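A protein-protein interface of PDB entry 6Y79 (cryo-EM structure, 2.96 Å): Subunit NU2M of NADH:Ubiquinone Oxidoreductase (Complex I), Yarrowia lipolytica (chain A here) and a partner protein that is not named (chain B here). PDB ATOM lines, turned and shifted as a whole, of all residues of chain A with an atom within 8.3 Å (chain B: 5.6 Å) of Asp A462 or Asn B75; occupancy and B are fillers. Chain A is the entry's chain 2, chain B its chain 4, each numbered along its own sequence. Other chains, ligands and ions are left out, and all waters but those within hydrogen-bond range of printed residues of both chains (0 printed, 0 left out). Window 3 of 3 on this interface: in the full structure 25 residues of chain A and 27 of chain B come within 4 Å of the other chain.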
ATOM      1  N   PHE A 307      16.894   4.515 -26.145  1.00  0.00           N
ATOM      2  CA  PHE A 307      17.036   3.799 -24.884  1.00  0.00           C
ATOM      3  C   PHE A 307      18.467   3.375 -24.662  1.00  0.00           C
ATOM      4  O   PHE A 307      19.038   3.613 -23.588  1.00  0.00           O
ATOM      5  CB  PHE A 307      16.141   2.565 -24.836  1.00  0.00           C
ATOM      6  CG  PHE A 307      16.198   1.850 -23.524  1.00  0.00           C
ATOM      7  CD1 PHE A 307      15.668   2.427 -22.388  1.00  0.00           C
ATOM      8  CD2 PHE A 307      16.805   0.617 -23.418  1.00  0.00           C
ATOM      9  CE1 PHE A 307      15.728   1.793 -21.178  1.00  0.00           C
ATOM     10  CE2 PHE A 307      16.867  -0.024 -22.211  1.00  0.00           C
ATOM     11  CZ  PHE A 307      16.329   0.567 -21.089  1.00  0.00           C
ATOM     12  N   ILE A 455      18.464  -3.131 -10.184  1.00  0.00           N
ATOM     13  CA  ILE A 455      17.181  -3.299  -9.511  1.00  0.00           C
ATOM     14  C   ILE A 455      16.093  -2.525 -10.238  1.00  0.00           C
ATOM     15  O   ILE A 455      14.996  -3.034 -10.486  1.00  0.00           O
ATOM     16  CB  ILE A 455      17.308  -2.845  -8.048  1.00  0.00           C
ATOM     17  CG1 ILE A 455      18.333  -3.709  -7.317  1.00  0.00           C
ATOM     18  CG2 ILE A 455      15.972  -2.844  -7.361  1.00  0.00           C
ATOM     19  CD1 ILE A 455      18.661  -3.223  -5.936  1.00  0.00           C
ATOM     20  N   TYR A 456      16.402  -1.297 -10.626  1.00  0.00           N
ATOM     21  CA  TYR A 456      15.417  -0.363 -11.138  1.00  0.00           C
ATOM     22  C   TYR A 456      15.251  -0.411 -12.648  1.00  0.00           C
ATOM     23  O   TYR A 456      14.691   0.531 -13.206  1.00  0.00           O
ATOM     24  CB  TYR A 456      15.790   1.053 -10.717  1.00  0.00           C
ATOM     25  CG  TYR A 456      15.735   1.274  -9.236  1.00  0.00           C
ATOM     26  CD1 TYR A 456      14.527   1.487  -8.603  1.00  0.00           C
ATOM     27  CD2 TYR A 456      16.887   1.268  -8.468  1.00  0.00           C
ATOM     28  CE1 TYR A 456      14.455   1.695  -7.253  1.00  0.00           C
ATOM     29  CE2 TYR A 456      16.828   1.470  -7.106  1.00  0.00           C
ATOM     30  CZ  TYR A 456      15.603   1.687  -6.508  1.00  0.00           C
ATOM     31  OH  TYR A 456      15.515   1.894  -5.157  1.00  0.00           O
ATOM     32  N   ASN A 457      15.706  -1.479 -13.311  1.00  0.00           N
ATOM     33  CA  ASN A 457      15.645  -1.554 -14.770  1.00  0.00           C
ATOM     34  C   ASN A 457      14.217  -1.543 -15.288  1.00  0.00           C
ATOM     35  O   ASN A 457      13.919  -0.878 -16.282  1.00  0.00           O
ATOM     36  CB  ASN A 457      16.346  -2.810 -15.275  1.00  0.00           C
ATOM     37  CG  ASN A 457      17.835  -2.672 -15.304  1.00  0.00           C
ATOM     38  OD1 ASN A 457      18.368  -1.587 -15.501  1.00  0.00           O
ATOM     39  ND2 ASN A 457      18.523  -3.779 -15.128  1.00  0.00           N
ATOM     40  N   SER A 458      13.312  -2.241 -14.613  1.00  0.00           N
ATOM     41  CA  SER A 458      11.942  -2.322 -15.105  1.00  0.00           C
ATOM     42  C   SER A 458      11.166  -1.040 -14.814  1.00  0.00           C
ATOM     43  O   SER A 458      10.336  -0.614 -15.630  1.00  0.00           O
ATOM     44  CB  SER A 458      11.258  -3.538 -14.499  1.00  0.00           C
ATOM     45  OG  SER A 458      11.216  -3.423 -13.095  1.00  0.00           O
ATOM     46  N   LEU A 459      11.432  -0.406 -13.661  1.00  0.00           N
ATOM     47  CA  LEU A 459      10.904   0.929 -13.381  1.00  0.00           C
ATOM     48  C   LEU A 459      11.342   1.927 -14.437  1.00  0.00           C
ATOM     49  O   LEU A 459      10.536   2.730 -14.926  1.00  0.00           O
ATOM     50  CB  LEU A 459      11.383   1.427 -12.020  1.00  0.00           C
ATOM     51  CG  LEU A 459      10.768   1.009 -10.692  1.00  0.00           C
ATOM     52  CD1 LEU A 459      11.162   1.981  -9.624  1.00  0.00           C
ATOM     53  CD2 LEU A 459       9.314   1.019 -10.803  1.00  0.00           C
ATOM     54  N   ILE A 460      12.618   1.871 -14.808  1.00  0.00           N
ATOM     55  CA  ILE A 460      13.181   2.806 -15.768  1.00  0.00           C
ATOM     56  C   ILE A 460      12.612   2.557 -17.157  1.00  0.00           C
ATOM     57  O   ILE A 460      12.320   3.504 -17.892  1.00  0.00           O
ATOM     58  CB  ILE A 460      14.715   2.702 -15.711  1.00  0.00           C
ATOM     59  CG1 ILE A 460      15.214   3.481 -14.506  1.00  0.00           C
ATOM     60  CG2 ILE A 460      15.385   3.218 -16.961  1.00  0.00           C
ATOM     61  CD1 ILE A 460      16.569   3.104 -14.094  1.00  0.00           C
ATOM     62  N   ILE A 461      12.379   1.294 -17.511  1.00  0.00           N
ATOM     63  CA  ILE A 461      11.775   0.990 -18.804  1.00  0.00           C
ATOM     64  C   ILE A 461      10.318   1.445 -18.855  1.00  0.00           C
ATOM     65  O   ILE A 461       9.864   1.945 -19.886  1.00  0.00           O
ATOM     66  CB  ILE A 461      11.950  -0.510 -19.117  1.00  0.00           C
ATOM     67  CG1 ILE A 461      13.404  -0.794 -19.469  1.00  0.00           C
ATOM     68  CG2 ILE A 461      11.126  -0.955 -20.302  1.00  0.00           C
ATOM     69  CD1 ILE A 461      13.756  -2.244 -19.456  1.00  0.00           C
ATOM     70  N   ASP A 462       9.585   1.375 -17.741  1.00  0.00           N
ATOM     71  CA  ASP A 462       8.200   1.851 -17.755  1.00  0.00           C
ATOM     72  C   ASP A 462       8.112   3.378 -17.854  1.00  0.00           C
ATOM     73  O   ASP A 462       7.291   3.921 -18.619  1.00  0.00           O
ATOM     74  CB  ASP A 462       7.476   1.347 -16.514  1.00  0.00           C
ATOM     75  CG  ASP A 462       7.150  -0.129 -16.598  1.00  0.00           C
ATOM     76  OD1 ASP A 462       7.113  -0.665 -17.721  1.00  0.00           O
ATOM     77  OD2 ASP A 462       6.912  -0.752 -15.545  1.00  0.00           O
ATOM     78  N   ILE A 463       8.961   4.086 -17.105  1.00  0.00           N
ATOM     79  CA  ILE A 463       8.996   5.547 -17.185  1.00  0.00           C
ATOM     80  C   ILE A 463       9.483   6.001 -18.564  1.00  0.00           C
ATOM     81  O   ILE A 463       9.006   7.007 -19.117  1.00  0.00           O
ATOM     82  CB  ILE A 463       9.863   6.091 -16.035  1.00  0.00           C
ATOM     83  CG1 ILE A 463       9.227   5.753 -14.692  1.00  0.00           C
ATOM     84  CG2 ILE A 463       9.989   7.566 -16.088  1.00  0.00           C
ATOM     85  CD1 ILE A 463      10.138   5.975 -13.522  1.00  0.00           C
ATOM     86  N   PHE A 464      10.410   5.243 -19.150  1.00  0.00           N
ATOM     87  CA  PHE A 464      10.791   5.421 -20.544  1.00  0.00           C
ATOM     88  C   PHE A 464       9.591   5.282 -21.462  1.00  0.00           C
ATOM     89  O   PHE A 464       9.462   6.029 -22.435  1.00  0.00           O
ATOM     90  CB  PHE A 464      11.850   4.373 -20.908  1.00  0.00           C
ATOM     91  CG  PHE A 464      12.379   4.477 -22.310  1.00  0.00           C
ATOM     92  CD1 PHE A 464      11.727   3.879 -23.394  1.00  0.00           C
ATOM     93  CD2 PHE A 464      13.542   5.150 -22.547  1.00  0.00           C
ATOM     94  CE1 PHE A 464      12.192   3.999 -24.650  1.00  0.00           C
ATOM     95  CE2 PHE A 464      14.028   5.235 -23.810  1.00  0.00           C
ATOM     96  CZ  PHE A 464      13.351   4.671 -24.863  1.00  0.00           C
ATOM     97  N   ASN A 465       8.767   4.258 -21.230  1.00  0.00           N
ATOM     98  CA  ASN A 465       7.662   3.955 -22.132  1.00  0.00           C
ATOM     99  C   ASN A 465       6.650   5.078 -22.150  1.00  0.00           C
ATOM    100  O   ASN A 465       5.999   5.322 -23.170  1.00  0.00           O
ATOM    101  CB  ASN A 465       6.977   2.661 -21.712  1.00  0.00           C
ATOM    102  CG  ASN A 465       7.779   1.446 -22.059  1.00  0.00           C
ATOM    103  OD1 ASN A 465       8.504   1.430 -23.050  1.00  0.00           O
ATOM    104  ND2 ASN A 465       7.662   0.412 -21.238  1.00  0.00           N
ATOM    105  N   VAL A 466       6.506   5.780 -21.027  1.00  0.00           N
ATOM    106  CA  VAL A 466       5.510   6.846 -21.013  1.00  0.00           C
ATOM    107  C   VAL A 466       6.088   8.160 -21.551  1.00  0.00           C
ATOM    108  O   VAL A 466       5.414   8.885 -22.293  1.00  0.00           O
ATOM    109  CB  VAL A 466       4.868   6.997 -19.616  1.00  0.00           C
ATOM    110  CG1 VAL A 466       5.842   7.435 -18.573  1.00  0.00           C
ATOM    111  CG2 VAL A 466       3.721   7.945 -19.675  1.00  0.00           C
ATOM    112  N   TYR A 467       7.341   8.504 -21.218  1.00  0.00           N
ATOM    113  CA  TYR A 467       7.736   9.873 -21.540  1.00  0.00           C
ATOM    114  C   TYR A 467       8.370  10.013 -22.908  1.00  0.00           C
ATOM    115  O   TYR A 467       8.588  11.135 -23.363  1.00  0.00           O
ATOM    116  CB  TYR A 467       8.691  10.431 -20.503  1.00  0.00           C
ATOM    117  CG  TYR A 467       8.030  10.723 -19.188  1.00  0.00           C
ATOM    118  CD1 TYR A 467       6.672  10.946 -19.095  1.00  0.00           C
ATOM    119  CD2 TYR A 467       8.765  10.777 -18.036  1.00  0.00           C
ATOM    120  CE1 TYR A 467       6.076  11.204 -17.883  1.00  0.00           C
ATOM    121  CE2 TYR A 467       8.181  11.041 -16.820  1.00  0.00           C
ATOM    122  CZ  TYR A 467       6.832  11.259 -16.754  1.00  0.00           C
ATOM    123  OH  TYR A 467       6.220  11.520 -15.554  1.00  0.00           O
ATOM    124  N   PHE A 468       8.725   8.917 -23.560  1.00  0.00           N
ATOM    125  CA  PHE A 468       9.327   9.008 -24.881  1.00  0.00           C
ATOM    126  C   PHE A 468       8.442   8.434 -25.954  1.00  0.00           C
ATOM    127  O   PHE A 468       8.768   8.567 -27.134  1.00  0.00           O
ATOM    128  CB  PHE A 468      10.677   8.296 -24.973  1.00  0.00           C
ATOM    129  CG  PHE A 468      11.790   8.886 -24.099  1.00  0.00           C
ATOM    130  CD1 PHE A 468      11.642   9.957 -23.264  1.00  0.00           C
ATOM    131  CD2 PHE A 468      13.011   8.384 -24.242  1.00  0.00           C
ATOM    132  CE1 PHE A 468      12.668  10.421 -22.508  1.00  0.00           C
ATOM    133  CE2 PHE A 468      14.057   8.826 -23.523  1.00  0.00           C
ATOM    134  CZ  PHE A 468      13.878   9.875 -22.657  1.00  0.00           C
ATOM    135  N   ASN A 469       7.377   7.742 -25.585  1.00  0.00           N
ATOM    136  CA  ASN A 469       6.449   7.201 -26.572  1.00  0.00           C
ATOM    137  C   ASN A 469       5.058   7.808 -26.394  1.00  0.00           C
ATOM    138  O   ASN A 469       4.404   7.596 -25.371  1.00  0.00           O
ATOM    139  CB  ASN A 469       6.364   5.674 -26.480  1.00  0.00           C
ATOM    140  CG  ASN A 469       7.728   5.005 -26.419  1.00  0.00           C
ATOM    141  OD1 ASN A 469       8.739   5.585 -26.794  1.00  0.00           O
ATOM    142  ND2 ASN A 469       7.754   3.766 -25.960  1.00  0.00           N
ATOM    143  N   GLU B  58       9.146 -14.074  -8.167  1.00  0.00           N
ATOM    144  CA  GLU B  58       9.629 -13.053  -9.082  1.00  0.00           C
ATOM    145  C   GLU B  58      10.366 -11.980  -8.301  1.00  0.00           C
ATOM    146  O   GLU B  58       9.884 -11.523  -7.264  1.00  0.00           O
ATOM    147  CB  GLU B  58       8.480 -12.427  -9.864  1.00  0.00           C
ATOM    148  CG  GLU B  58       8.930 -11.504 -10.966  1.00  0.00           C
ATOM    149  CD  GLU B  58       7.774 -10.864 -11.692  1.00  0.00           C
ATOM    150  OE1 GLU B  58       6.613 -11.168 -11.351  1.00  0.00           O
ATOM    151  OE2 GLU B  58       8.024 -10.051 -12.601  1.00  0.00           O
ATOM    152  N   PHE B  60      12.460  -8.147  -8.595  1.00  0.00           N
ATOM    153  CA  PHE B  60      12.704  -6.895  -9.321  1.00  0.00           C
ATOM    154  C   PHE B  60      11.625  -6.602 -10.361  1.00  0.00           C
ATOM    155  O   PHE B  60      11.910  -6.151 -11.468  1.00  0.00           O
ATOM    156  CB  PHE B  60      14.098  -6.888  -9.950  1.00  0.00           C
ATOM    157  CG  PHE B  60      15.179  -7.178  -8.973  1.00  0.00           C
ATOM    158  CD1 PHE B  60      15.331  -6.374  -7.873  1.00  0.00           C
ATOM    159  CD2 PHE B  60      16.022  -8.257  -9.132  1.00  0.00           C
ATOM    160  CE1 PHE B  60      16.305  -6.630  -6.947  1.00  0.00           C
ATOM    161  CE2 PHE B  60      17.004  -8.517  -8.209  1.00  0.00           C
ATOM    162  CZ  PHE B  60      17.146  -7.701  -7.120  1.00  0.00           C
ATOM    163  N   ASN B  61      10.376  -6.869 -10.000  1.00  0.00           N
ATOM    164  CA  ASN B  61       9.243  -6.400 -10.775  1.00  0.00           C
ATOM    165  C   ASN B  61       9.110  -4.894 -10.594  1.00  0.00           C
ATOM    166  O   ASN B  61       9.642  -4.318  -9.654  1.00  0.00           O
ATOM    167  CB  ASN B  61       7.970  -7.118 -10.327  1.00  0.00           C
ATOM    168  CG  ASN B  61       6.867  -7.046 -11.348  1.00  0.00           C
ATOM    169  OD1 ASN B  61       7.036  -6.481 -12.409  1.00  0.00           O
ATOM    170  ND2 ASN B  61       5.726  -7.623 -11.027  1.00  0.00           N
ATOM    171  N   SER B  62       8.402  -4.241 -11.511  1.00  0.00           N
ATOM    172  CA  SER B  62       8.288  -2.788 -11.422  1.00  0.00           C
ATOM    173  C   SER B  62       7.323  -2.374 -10.318  1.00  0.00           C
ATOM    174  O   SER B  62       7.561  -1.390  -9.613  1.00  0.00           O
ATOM    175  CB  SER B  62       7.861  -2.208 -12.766  1.00  0.00           C
ATOM    176  OG  SER B  62       6.568  -2.637 -13.123  1.00  0.00           O
ATOM    177  N   ILE B  73       1.123  -8.149 -14.524  1.00  0.00           N
ATOM    178  CA  ILE B  73       2.143  -7.938 -15.539  1.00  0.00           C
ATOM    179  C   ILE B  73       3.496  -8.200 -14.894  1.00  0.00           C
ATOM    180  O   ILE B  73       3.711  -7.876 -13.721  1.00  0.00           O
ATOM    181  CB  ILE B  73       2.038  -6.525 -16.160  1.00  0.00           C
ATOM    182  CG1 ILE B  73       2.802  -6.447 -17.460  1.00  0.00           C
ATOM    183  CG2 ILE B  73       2.481  -5.394 -15.219  1.00  0.00           C
ATOM    184  CD1 ILE B  73       2.406  -5.268 -18.259  1.00  0.00           C
ATOM    185  N   SER B  74       4.368  -8.888 -15.611  1.00  0.00           N
ATOM    186  CA  SER B  74       5.593  -9.386 -15.017  1.00  0.00           C
ATOM    187  C   SER B  74       6.743  -9.115 -15.960  1.00  0.00           C
ATOM    188  O   SER B  74       6.780  -9.657 -17.067  1.00  0.00           O
ATOM    189  CB  SER B  74       5.490 -10.871 -14.714  1.00  0.00           C
ATOM    190  OG  SER B  74       5.365 -11.601 -15.915  1.00  0.00           O
ATOM    191  N   ASN B  75       7.681  -8.283 -15.515  1.00  0.00           N
ATOM    192  CA  ASN B  75       8.869  -7.997 -16.295  1.00  0.00           C
ATOM    193  C   ASN B  75      10.147  -8.086 -15.473  1.00  0.00           C
ATOM    194  O   ASN B  75      11.180  -7.570 -15.904  1.00  0.00           O
ATOM    195  CB  ASN B  75       8.761  -6.623 -16.963  1.00  0.00           C
ATOM    196  CG  ASN B  75       8.372  -5.520 -15.997  1.00  0.00           C
ATOM    197  OD1 ASN B  75       8.269  -5.728 -14.799  1.00  0.00           O
ATOM    198  ND2 ASN B  75       8.158  -4.330 -16.529  1.00  0.00           N
ATOM    199  N   GLY B  76      10.111  -8.728 -14.311  1.00  0.00           N
ATOM    200  CA  GLY B  76      11.319  -8.928 -13.538  1.00  0.00           C
ATOM    201  C   GLY B  76      12.044 -10.206 -13.897  1.00  0.00           C
ATOM    202  O   GLY B  76      12.068 -10.611 -15.060  1.00  0.00           O
ATOM    203  N   LEU B  77      12.634 -10.853 -12.897  1.00  0.00           N
ATOM    204  CA  LEU B  77      13.377 -12.095 -13.059  1.00  0.00           C
ATOM    205  C   LEU B  77      12.625 -13.203 -12.344  1.00  0.00           C
ATOM    206  O   LEU B  77      12.353 -13.093 -11.146  1.00  0.00           O
ATOM    207  CB  LEU B  77      14.787 -11.959 -12.493  1.00  0.00           C
ATOM    208  CG  LEU B  77      15.587 -10.745 -12.953  1.00  0.00           C
ATOM    209  CD1 LEU B  77      16.817 -10.574 -12.093  1.00  0.00           C
ATOM    210  CD2 LEU B  77      15.970 -10.878 -14.413  1.00  0.00           C
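OG of Ser A458 is in hydrogen-bond range of O of Phe B60 (3.3 Å).
The backbone NH of Ser B62 is in hydrogen-bond range of the side-chain hydroxyl of Ser A458 (3.3 Å).
The side-chain carboxylate (OD2) of Asp A462 sits at hydrogen-bond distance from the side-chain hydroxyl (OG) of Ser B62.
OD1 of Asn B61 sits close to OD1 of Asn B75, 2.8 Å away.
The backbone carbonyl oxygen (O) of Ile B73 is in hydrogen-bond range of the side-chain amide nitrogen (ND2) of Asn B61 (3.4 Å).
The backbone NH of Asn B75 is in hydrogen-bond range of the side-chain carboxylate of Glu B58, 3.4 Å away.
Among the printed residues, merely in contact across the chains: Leu A459 with Ser B62 (3.2 Å), Ile A455 with Phe B60 (3.6 Å), Ser A458 with Asn B61 (3.6 Å), Ser A458 with Asn B75 (3.7 Å) and Asp A462 with Asn B75 (3.9 Å).
Printed residues of chain B within 4 Å of Ile A455: Phe B60 (3.6 Å).
Of the printed residues of chain B, Leu A459 touches Ser B62 (3.2 Å).
Printed residues of chain B within 4 Å of Asp A462: Ser B62 and Asn B75.
No residue of chain A comes within 4 Å of Ser B74.
Asn B75 touches just these residues of chain A: Ser A458 (3.7 Å) and Asp A462 (3.9 Å).
Gly B76 touches none of the printed residues of chain A.
The nearest printed residue of chain B that does not touch Asp A462 is Ile B73 (6.4 Å).
The nearest printed residue of chain A that does not touch Phe B60 is Tyr A456 (5.9 Å).
Of the 16 printed residues of chain A, 4 touch a printed residue of chain B.
Along chain A the printed residues that touch a printed residue of chain B span positions 455 to 462.
Among the printed residues, 8 pairs touch across the chains.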
